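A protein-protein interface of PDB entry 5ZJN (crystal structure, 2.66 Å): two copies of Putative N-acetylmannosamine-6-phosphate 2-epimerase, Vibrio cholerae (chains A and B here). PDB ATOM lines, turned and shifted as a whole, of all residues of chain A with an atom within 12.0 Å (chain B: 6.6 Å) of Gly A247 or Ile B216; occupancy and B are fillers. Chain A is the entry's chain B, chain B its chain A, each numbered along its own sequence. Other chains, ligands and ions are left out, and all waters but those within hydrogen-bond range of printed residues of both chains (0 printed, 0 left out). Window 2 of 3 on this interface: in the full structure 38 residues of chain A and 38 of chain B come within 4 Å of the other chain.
Trp A238 touches none of the printed residues of chain B. Printed residues of chain B within 4 Å of Ala A242: Ala B213 (3.4 Å). Of the printed residues of chain B, Thr A243 touches Gly B34 (2.8 Å), Gln B35 (3.8 Å), Ala B212 (3.5 Å) and Val B223 (3.6 Å). Of the printed residues of chain B, Gln A244 touches Gly B34 and Gln B35. Of the printed residues of chain B, Ala A246 touches Ala B213 (3.7 Å). Of the printed residues of chain B, Gly A247 touches Ile B216 (3.99 Å). Printed residues of chain A within 4 Å of Gln B35: Asn A240, Thr A243 and Gln A244. Ala B212 touches just one residue of chain A: Thr A243 (3.5 Å). Ala B215 touches none of the printed residues of chain A. No residue of chain A comes within 4 Å of Ser B218. No residue of chain A comes within 4 Å of Gly B219. No residue of chain A comes within 4 Å of Ala B220. No residue of chain A comes within 4 Å of Ala B222. Of the printed residues of chain A, Val B223 touches Thr A243. The nearest printed residue of chain B that does not touch Gly A247 is Asn B33 (4.04 Å).
Of the 19 printed residues of chain B, 6 touch a printed residue of chain A. Printed residues of chain A that touch a printed residue of chain B: Asn A240, Ala A242, Thr A243, Gln A244, Ala A246 and Gly A247. Hydrophobic or aromatic side chains of chain A that line the printed part of chain B: Ala A246.
Among the printed residues, merely in contact across the chains: Ala A242 with Ala B213 (3.4 Å), Thr A243 with Ala B212 (3.5 Å), Thr A243 with Val B223 (3.6 Å), Ala A246 with Ala B213 (3.7 Å), Thr A243 with Gln B35 (3.8 Å) and Gly A247 with Ile B216 (3.99 Å).
No position is printed for both chains. Of the 10 pairs that touch across the chains among the printed residues, none has its exchanged pair printed and touching as well.
The side-chain hydroxyl (OG1) of Thr A243 sits close to the backbone carbonyl oxygen (O) of Asn A240, at 3.4 Å. The backbone carbonyl oxygen of Phe A239 is in hydrogen-bond range of the side-chain hydroxyl of Thr A243, 3.2 Å away. The backbone NH of Gly B34 is in hydrogen-bond range of the backbone carbonyl oxygen of Val B221 (2.8 Å). O of Gln B35 is in hydrogen-bond range of N of Val B223 (3.2 Å).
The backbone carbonyl oxygen of Gly B34 lies within hydrogen-bond range of the side-chain hydroxyl of Thr A243, 2.8 Å away. OE1 of Gln B35 lies close to OD1 of Asn A240 (3.3 Å). O of Gly B34 is in hydrogen-bond range of N of Gln A244. NE2 of Gln B35 sits at hydrogen-bond distance from OE1 of Gln A244, at 2.8 Å.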
ATOM      1  N   TRP A 238      -1.413 -14.223 -32.289  1.00  0.00           N
ATOM      2  CA  TRP A 238      -1.074 -12.924 -31.712  1.00  0.00           C
ATOM      3  C   TRP A 238      -0.441 -13.075 -30.323  1.00  0.00           C
ATOM      4  O   TRP A 238       0.498 -12.348 -29.974  1.00  0.00           O
ATOM      5  CB  TRP A 238      -2.320 -12.044 -31.632  1.00  0.00           C
ATOM      6  CG  TRP A 238      -2.782 -11.474 -32.924  1.00  0.00           C
ATOM      7  CD1 TRP A 238      -2.103 -11.451 -34.115  1.00  0.00           C
ATOM      8  CD2 TRP A 238      -4.040 -10.823 -33.165  1.00  0.00           C
ATOM      9  NE1 TRP A 238      -2.862 -10.830 -35.073  1.00  0.00           N
ATOM     10  CE2 TRP A 238      -4.055 -10.437 -34.521  1.00  0.00           C
ATOM     11  CE3 TRP A 238      -5.155 -10.530 -32.365  1.00  0.00           C
ATOM     12  CZ2 TRP A 238      -5.139  -9.770 -35.098  1.00  0.00           C
ATOM     13  CZ3 TRP A 238      -6.239  -9.868 -32.944  1.00  0.00           C
ATOM     14  CH2 TRP A 238      -6.220  -9.498 -34.297  1.00  0.00           C
ATOM     15  N   PHE A 239      -0.959 -14.008 -29.515  1.00  0.00           N
ATOM     16  CA  PHE A 239      -0.463 -14.190 -28.157  1.00  0.00           C
ATOM     17  C   PHE A 239       0.901 -14.885 -28.139  1.00  0.00           C
ATOM     18  O   PHE A 239       1.846 -14.395 -27.509  1.00  0.00           O
ATOM     19  CB  PHE A 239      -1.494 -14.963 -27.326  1.00  0.00           C
ATOM     20  CG  PHE A 239      -2.595 -14.100 -26.762  1.00  0.00           C
ATOM     21  CD1 PHE A 239      -3.641 -13.651 -27.557  1.00  0.00           C
ATOM     22  CD2 PHE A 239      -2.557 -13.701 -25.427  1.00  0.00           C
ATOM     23  CE1 PHE A 239      -4.634 -12.851 -27.025  1.00  0.00           C
ATOM     24  CE2 PHE A 239      -3.549 -12.889 -24.900  1.00  0.00           C
ATOM     25  CZ  PHE A 239      -4.591 -12.469 -25.701  1.00  0.00           C
ATOM     26  N   ASN A 240       1.025 -16.022 -28.838  1.00  0.00           N
ATOM     27  CA  ASN A 240       2.297 -16.738 -28.863  1.00  0.00           C
ATOM     28  C   ASN A 240       3.396 -15.893 -29.479  1.00  0.00           C
ATOM     29  O   ASN A 240       4.559 -16.000 -29.085  1.00  0.00           O
ATOM     30  CB  ASN A 240       2.144 -18.062 -29.601  1.00  0.00           C
ATOM     31  CG  ASN A 240       1.973 -19.241 -28.655  1.00  0.00           C
ATOM     32  OD1 ASN A 240       2.351 -19.173 -27.483  1.00  0.00           O
ATOM     33  ND2 ASN A 240       1.388 -20.324 -29.156  1.00  0.00           N
ATOM     34  N   ASN A 241       3.047 -15.056 -30.449  1.00  0.00           N
ATOM     35  CA  ASN A 241       4.040 -14.195 -31.080  1.00  0.00           C
ATOM     36  C   ASN A 241       4.720 -13.291 -30.051  1.00  0.00           C
ATOM     37  O   ASN A 241       5.933 -13.070 -30.115  1.00  0.00           O
ATOM     38  CB  ASN A 241       3.349 -13.399 -32.196  1.00  0.00           C
ATOM     39  CG  ASN A 241       4.276 -12.446 -32.929  1.00  0.00           C
ATOM     40  OD1 ASN A 241       4.579 -11.350 -32.452  1.00  0.00           O
ATOM     41  ND2 ASN A 241       4.735 -12.866 -34.104  1.00  0.00           N
ATOM     42  N   ALA A 242       3.954 -12.794 -29.079  1.00  0.00           N
ATOM     43  CA  ALA A 242       4.427 -11.859 -28.065  1.00  0.00           C
ATOM     44  C   ALA A 242       5.032 -12.545 -26.836  1.00  0.00           C
ATOM     45  O   ALA A 242       5.939 -11.993 -26.204  1.00  0.00           O
ATOM     46  CB  ALA A 242       3.270 -10.938 -27.641  1.00  0.00           C
ATOM     47  N   THR A 243       4.518 -13.719 -26.470  1.00  0.00           N
ATOM     48  CA  THR A 243       5.092 -14.472 -25.370  1.00  0.00           C
ATOM     49  C   THR A 243       6.371 -15.172 -25.792  1.00  0.00           C
ATOM     50  O   THR A 243       7.296 -15.314 -24.985  1.00  0.00           O
ATOM     51  CB  THR A 243       4.087 -15.492 -24.834  1.00  0.00           C
ATOM     52  OG1 THR A 243       3.749 -16.433 -25.855  1.00  0.00           O
ATOM     53  CG2 THR A 243       2.861 -14.808 -24.304  1.00  0.00           C
ATOM     54  N   GLN A 244       6.424 -15.647 -27.039  1.00  0.00           N
ATOM     55  CA  GLN A 244       7.635 -16.296 -27.525  1.00  0.00           C
ATOM     56  C   GLN A 244       8.732 -15.276 -27.807  1.00  0.00           C
ATOM     57  O   GLN A 244       9.905 -15.522 -27.502  1.00  0.00           O
ATOM     58  CB  GLN A 244       7.324 -17.134 -28.760  1.00  0.00           C
ATOM     59  CG  GLN A 244       6.618 -18.446 -28.440  1.00  0.00           C
ATOM     60  CD  GLN A 244       5.972 -19.078 -29.663  1.00  0.00           C
ATOM     61  OE1 GLN A 244       5.106 -19.954 -29.547  1.00  0.00           O
ATOM     62  NE2 GLN A 244       6.366 -18.618 -30.843  1.00  0.00           N
ATOM     63  N   ALA A 245       8.376 -14.117 -28.366  1.00  0.00           N
ATOM     64  CA  ALA A 245       9.386 -13.083 -28.578  1.00  0.00           C
ATOM     65  C   ALA A 245       9.983 -12.625 -27.253  1.00  0.00           C
ATOM     66  O   ALA A 245      11.182 -12.348 -27.164  1.00  0.00           O
ATOM     67  CB  ALA A 245       8.792 -11.899 -29.343  1.00  0.00           C
ATOM     68  N   ALA A 246       9.157 -12.545 -26.212  1.00  0.00           N
ATOM     69  CA  ALA A 246       9.667 -12.229 -24.889  1.00  0.00           C
ATOM     70  C   ALA A 246      10.571 -13.345 -24.375  1.00  0.00           C
ATOM     71  O   ALA A 246      11.623 -13.079 -23.786  1.00  0.00           O
ATOM     72  CB  ALA A 246       8.494 -11.975 -23.938  1.00  0.00           C
ATOM     73  N   GLY A 247      10.201 -14.596 -24.643  1.00  0.00           N
ATOM     74  CA  GLY A 247      10.934 -15.763 -24.194  1.00  0.00           C
ATOM     75  C   GLY A 247      12.255 -16.016 -24.898  1.00  0.00           C
ATOM     76  O   GLY A 247      12.799 -17.123 -24.819  1.00  0.00           O
ATOM     77  N   GLU A 248      12.780 -15.014 -25.601  1.00  0.00           N
ATOM     78  CA  GLU A 248      14.096 -15.085 -26.230  1.00  0.00           C
ATOM     79  C   GLU A 248      14.989 -14.191 -25.386  1.00  0.00           C
ATOM     80  O   GLU A 248      15.241 -13.029 -25.710  1.00  0.00           O
ATOM     81  CB  GLU A 248      14.100 -14.650 -27.715  1.00  0.00           C
ATOM     82  CG  GLU A 248      13.336 -15.557 -28.652  1.00  0.00           C
ATOM     83  CD  GLU A 248      13.642 -15.271 -30.114  1.00  0.00           C
ATOM     84  OE1 GLU A 248      14.602 -14.518 -30.392  1.00  0.00           O
ATOM     85  OE2 GLU A 248      12.927 -15.802 -30.990  1.00  0.00           O
ATOM     86  N   ARG A 249      15.457 -14.755 -24.281  1.00  0.00           N
ATOM     87  CA  ARG A 249      16.154 -14.013 -23.248  1.00  0.00           C
ATOM     88  C   ARG A 249      16.680 -15.009 -22.229  1.00  0.00           C
ATOM     89  O   ARG A 249      16.352 -16.195 -22.279  1.00  0.00           O
ATOM     90  CB  ARG A 249      15.218 -12.994 -22.589  1.00  0.00           C
ATOM     91  CG  ARG A 249      15.913 -11.832 -21.897  1.00  0.00           C
ATOM     92  CD  ARG A 249      14.900 -10.772 -21.492  1.00  0.00           C
ATOM     93  NE  ARG A 249      15.546  -9.589 -20.929  1.00  0.00           N
ATOM     94  CZ  ARG A 249      15.453  -9.218 -19.656  1.00  0.00           C
ATOM     95  NH1 ARG A 249      14.742  -9.945 -18.807  1.00  0.00           N
ATOM     96  NH2 ARG A 249      16.075  -8.120 -19.241  1.00  0.00           N
ATOM     97  N   LEU B  32       7.351 -25.630 -22.613  1.00  0.00           N
ATOM     98  CA  LEU B  32       6.377 -24.575 -22.364  1.00  0.00           C
ATOM     99  C   LEU B  32       6.998 -23.197 -22.213  1.00  0.00           C
ATOM    100  O   LEU B  32       6.279 -22.251 -21.878  1.00  0.00           O
ATOM    101  CB  LEU B  32       5.565 -24.877 -21.107  1.00  0.00           C
ATOM    102  CG  LEU B  32       4.685 -26.122 -21.120  1.00  0.00           C
ATOM    103  CD1 LEU B  32       3.999 -26.271 -19.769  1.00  0.00           C
ATOM    104  CD2 LEU B  32       3.657 -26.086 -22.248  1.00  0.00           C
ATOM    105  N   ASN B  33       8.304 -23.069 -22.402  1.00  0.00           N
ATOM    106  CA  ASN B  33       8.971 -21.795 -22.173  1.00  0.00           C
ATOM    107  C   ASN B  33       8.588 -20.781 -23.247  1.00  0.00           C
ATOM    108  O   ASN B  33       8.747 -21.034 -24.443  1.00  0.00           O
ATOM    109  CB  ASN B  33      10.489 -22.010 -22.116  1.00  0.00           C
ATOM    110  CG  ASN B  33      11.269 -20.713 -22.060  1.00  0.00           C
ATOM    111  OD1 ASN B  33      12.269 -20.552 -22.759  1.00  0.00           O
ATOM    112  ND2 ASN B  33      10.829 -19.788 -21.216  1.00  0.00           N
ATOM    113  N   GLY B  34       8.112 -19.617 -22.815  1.00  0.00           N
ATOM    114  CA  GLY B  34       7.652 -18.574 -23.717  1.00  0.00           C
ATOM    115  C   GLY B  34       6.319 -18.826 -24.400  1.00  0.00           C
ATOM    116  O   GLY B  34       5.933 -18.049 -25.275  1.00  0.00           O
ATOM    117  N   GLN B  35       5.582 -19.851 -23.978  1.00  0.00           N
ATOM    118  CA  GLN B  35       4.342 -20.256 -24.612  1.00  0.00           C
ATOM    119  C   GLN B  35       3.100 -19.648 -23.969  1.00  0.00           C
ATOM    120  O   GLN B  35       3.047 -19.357 -22.768  1.00  0.00           O
ATOM    121  CB  GLN B  35       4.200 -21.780 -24.598  1.00  0.00           C
ATOM    122  CG  GLN B  35       5.150 -22.509 -25.541  1.00  0.00           C
ATOM    123  CD  GLN B  35       4.983 -22.079 -26.992  1.00  0.00           C
ATOM    124  OE1 GLN B  35       3.876 -22.048 -27.528  1.00  0.00           O
ATOM    125  NE2 GLN B  35       6.085 -21.721 -27.620  1.00  0.00           N
ATOM    126  N   PHE B 187       0.872  -9.041 -11.428  1.00  0.00           N
ATOM    127  CA  PHE B 187       2.250  -9.280 -11.825  1.00  0.00           C
ATOM    128  C   PHE B 187       3.175  -9.513 -10.642  1.00  0.00           C
ATOM    129  O   PHE B 187       4.204 -10.182 -10.792  1.00  0.00           O
ATOM    130  CB  PHE B 187       2.773  -8.110 -12.648  1.00  0.00           C
ATOM    131  CG  PHE B 187       2.128  -7.983 -13.971  1.00  0.00           C
ATOM    132  CD1 PHE B 187       2.501  -8.808 -15.019  1.00  0.00           C
ATOM    133  CD2 PHE B 187       1.126  -7.056 -14.176  1.00  0.00           C
ATOM    134  CE1 PHE B 187       1.883  -8.695 -16.256  1.00  0.00           C
ATOM    135  CE2 PHE B 187       0.516  -6.940 -15.409  1.00  0.00           C
ATOM    136  CZ  PHE B 187       0.900  -7.764 -16.446  1.00  0.00           C
ATOM    137  N   ALA B 202       1.834 -17.931 -15.089  1.00  0.00           N
ATOM    138  CA  ALA B 202       0.969 -16.769 -14.943  1.00  0.00           C
ATOM    139  C   ALA B 202      -0.403 -17.046 -15.586  1.00  0.00           C
ATOM    140  O   ALA B 202      -0.497 -17.437 -16.752  1.00  0.00           O
ATOM    141  CB  ALA B 202       1.629 -15.534 -15.552  1.00  0.00           C
ATOM    142  N   LEU B 211       0.039  -7.811 -22.353  1.00  0.00           N
ATOM    143  CA  LEU B 211      -0.018  -8.214 -20.953  1.00  0.00           C
ATOM    144  C   LEU B 211       0.573  -9.607 -20.740  1.00  0.00           C
ATOM    145  O   LEU B 211       1.227  -9.859 -19.717  1.00  0.00           O
ATOM    146  CB  LEU B 211      -1.450  -8.141 -20.433  1.00  0.00           C
ATOM    147  CG  LEU B 211      -2.012  -6.731 -20.260  1.00  0.00           C
ATOM    148  CD1 LEU B 211      -3.463  -6.805 -19.845  1.00  0.00           C
ATOM    149  CD2 LEU B 211      -1.203  -5.957 -19.240  1.00  0.00           C
ATOM    150  N   ALA B 212       0.338 -10.527 -21.682  1.00  0.00           N
ATOM    151  CA  ALA B 212       0.930 -11.855 -21.589  1.00  0.00           C
ATOM    152  C   ALA B 212       2.432 -11.837 -21.865  1.00  0.00           C
ATOM    153  O   ALA B 212       3.133 -12.779 -21.490  1.00  0.00           O
ATOM    154  CB  ALA B 212       0.219 -12.813 -22.548  1.00  0.00           C
ATOM    155  N   ALA B 213       2.926 -10.822 -22.575  1.00  0.00           N
ATOM    156  CA  ALA B 213       4.359 -10.702 -22.815  1.00  0.00           C
ATOM    157  C   ALA B 213       5.101 -10.187 -21.585  1.00  0.00           C
ATOM    158  O   ALA B 213       6.227 -10.616 -21.308  1.00  0.00           O
ATOM    159  CB  ALA B 213       4.608  -9.787 -24.016  1.00  0.00           C
ATOM    160  N   LYS B 214       4.489  -9.261 -20.843  1.00  0.00           N
ATOM    161  CA  LYS B 214       5.110  -8.749 -19.628  1.00  0.00           C
ATOM    162  C   LYS B 214       5.068  -9.770 -18.496  1.00  0.00           C
ATOM    163  O   LYS B 214       5.883  -9.686 -17.572  1.00  0.00           O
ATOM    164  CB  LYS B 214       4.457  -7.427 -19.210  1.00  0.00           C
ATOM    165  CG  LYS B 214       4.456  -6.406 -20.340  1.00  0.00           C
ATOM    166  CD  LYS B 214       4.691  -4.981 -19.903  1.00  0.00           C
ATOM    167  CE  LYS B 214       6.179  -4.759 -19.715  1.00  0.00           C
ATOM    168  NZ  LYS B 214       6.862  -5.030 -21.009  1.00  0.00           N
ATOM    169  N   ALA B 215       4.131 -10.720 -18.545  1.00  0.00           N
ATOM    170  CA  ALA B 215       4.152 -11.835 -17.606  1.00  0.00           C
ATOM    171  C   ALA B 215       5.412 -12.675 -17.781  1.00  0.00           C
ATOM    172  O   ALA B 215       6.021 -13.107 -16.796  1.00  0.00           O
ATOM    173  CB  ALA B 215       2.910 -12.703 -17.783  1.00  0.00           C
ATOM    174  N   ILE B 216       5.810 -12.934 -19.033  1.00  0.00           N
ATOM    175  CA  ILE B 216       7.007 -13.739 -19.274  1.00  0.00           C
ATOM    176  C   ILE B 216       8.251 -13.023 -18.758  1.00  0.00           C
ATOM    177  O   ILE B 216       9.092 -13.631 -18.087  1.00  0.00           O
ATOM    178  CB  ILE B 216       7.130 -14.105 -20.763  1.00  0.00           C
ATOM    179  CG1 ILE B 216       5.965 -14.993 -21.146  1.00  0.00           C
ATOM    180  CG2 ILE B 216       8.470 -14.818 -21.052  1.00  0.00           C
ATOM    181  CD1 ILE B 216       5.989 -16.324 -20.446  1.00  0.00           C
ATOM    182  N   GLU B 217       8.386 -11.726 -19.060  1.00  0.00           N
ATOM    183  CA  GLU B 217       9.507 -10.972 -18.511  1.00  0.00           C
ATOM    184  C   GLU B 217       9.335 -10.716 -17.020  1.00  0.00           C
ATOM    185  O   GLU B 217      10.306 -10.393 -16.339  1.00  0.00           O
ATOM    186  CB  GLU B 217       9.714  -9.667 -19.273  1.00  0.00           C
ATOM    187  CG  GLU B 217       8.528  -8.781 -19.402  1.00  0.00           C
ATOM    188  CD  GLU B 217       8.703  -7.782 -20.542  1.00  0.00           C
ATOM    189  OE1 GLU B 217       9.867  -7.434 -20.838  1.00  0.00           O
ATOM    190  OE2 GLU B 217       7.687  -7.366 -21.159  1.00  0.00           O
ATOM    191  N   SER B 218       8.119 -10.846 -16.507  1.00  0.00           N
ATOM    192  CA  SER B 218       7.925 -10.872 -15.070  1.00  0.00           C
ATOM    193  C   SER B 218       8.478 -12.151 -14.465  1.00  0.00           C
ATOM    194  O   SER B 218       8.467 -12.289 -13.241  1.00  0.00           O
ATOM    195  CB  SER B 218       6.434 -10.743 -14.736  1.00  0.00           C
ATOM    196  OG  SER B 218       5.980  -9.403 -14.838  1.00  0.00           O
ATOM    197  N   GLY B 219       8.857 -13.122 -15.291  1.00  0.00           N
ATOM    198  CA  GLY B 219       9.500 -14.329 -14.817  1.00  0.00           C
ATOM    199  C   GLY B 219       8.764 -15.612 -15.104  1.00  0.00           C
ATOM    200  O   GLY B 219       9.303 -16.688 -14.813  1.00  0.00           O
ATOM    201  N   ALA B 220       7.564 -15.563 -15.667  1.00  0.00           N
ATOM    202  CA  ALA B 220       6.796 -16.778 -15.903  1.00  0.00           C
ATOM    203  C   ALA B 220       7.444 -17.638 -16.981  1.00  0.00           C
ATOM    204  O   ALA B 220       8.076 -17.138 -17.912  1.00  0.00           O
ATOM    205  CB  ALA B 220       5.344 -16.442 -16.294  1.00  0.00           C
ATOM    206  N   VAL B 221       7.311 -18.951 -16.810  1.00  0.00           N
ATOM    207  CA  VAL B 221       7.719 -19.890 -17.846  1.00  0.00           C
ATOM    208  C   VAL B 221       6.732 -19.851 -19.000  1.00  0.00           C
ATOM    209  O   VAL B 221       7.111 -19.820 -20.178  1.00  0.00           O
ATOM    210  CB  VAL B 221       7.800 -21.309 -17.256  1.00  0.00           C
ATOM    211  CG1 VAL B 221       7.970 -22.351 -18.372  1.00  0.00           C
ATOM    212  CG2 VAL B 221       8.890 -21.398 -16.266  1.00  0.00           C
ATOM    213  N   ALA B 222       5.449 -19.869 -18.661  1.00  0.00           N
ATOM    214  CA  ALA B 222       4.348 -19.820 -19.593  1.00  0.00           C
ATOM    215  C   ALA B 222       3.254 -18.962 -18.983  1.00  0.00           C
ATOM    216  O   ALA B 222       3.318 -18.567 -17.818  1.00  0.00           O
ATOM    217  CB  ALA B 222       3.836 -21.230 -19.909  1.00  0.00           C
ATOM    218  N   VAL B 223       2.232 -18.692 -19.781  1.00  0.00           N
ATOM    219  CA  VAL B 223       1.078 -17.908 -19.364  1.00  0.00           C
ATOM    220  C   VAL B 223      -0.167 -18.575 -19.929  1.00  0.00           C
ATOM    221  O   VAL B 223      -0.160 -19.071 -21.060  1.00  0.00           O
ATOM    222  CB  VAL B 223       1.189 -16.432 -19.811  1.00  0.00           C
ATOM    223  CG1 VAL B 223       1.599 -16.338 -21.266  1.00  0.00           C
ATOM    224  CG2 VAL B 223      -0.141 -15.696 -19.595  1.00  0.00           C
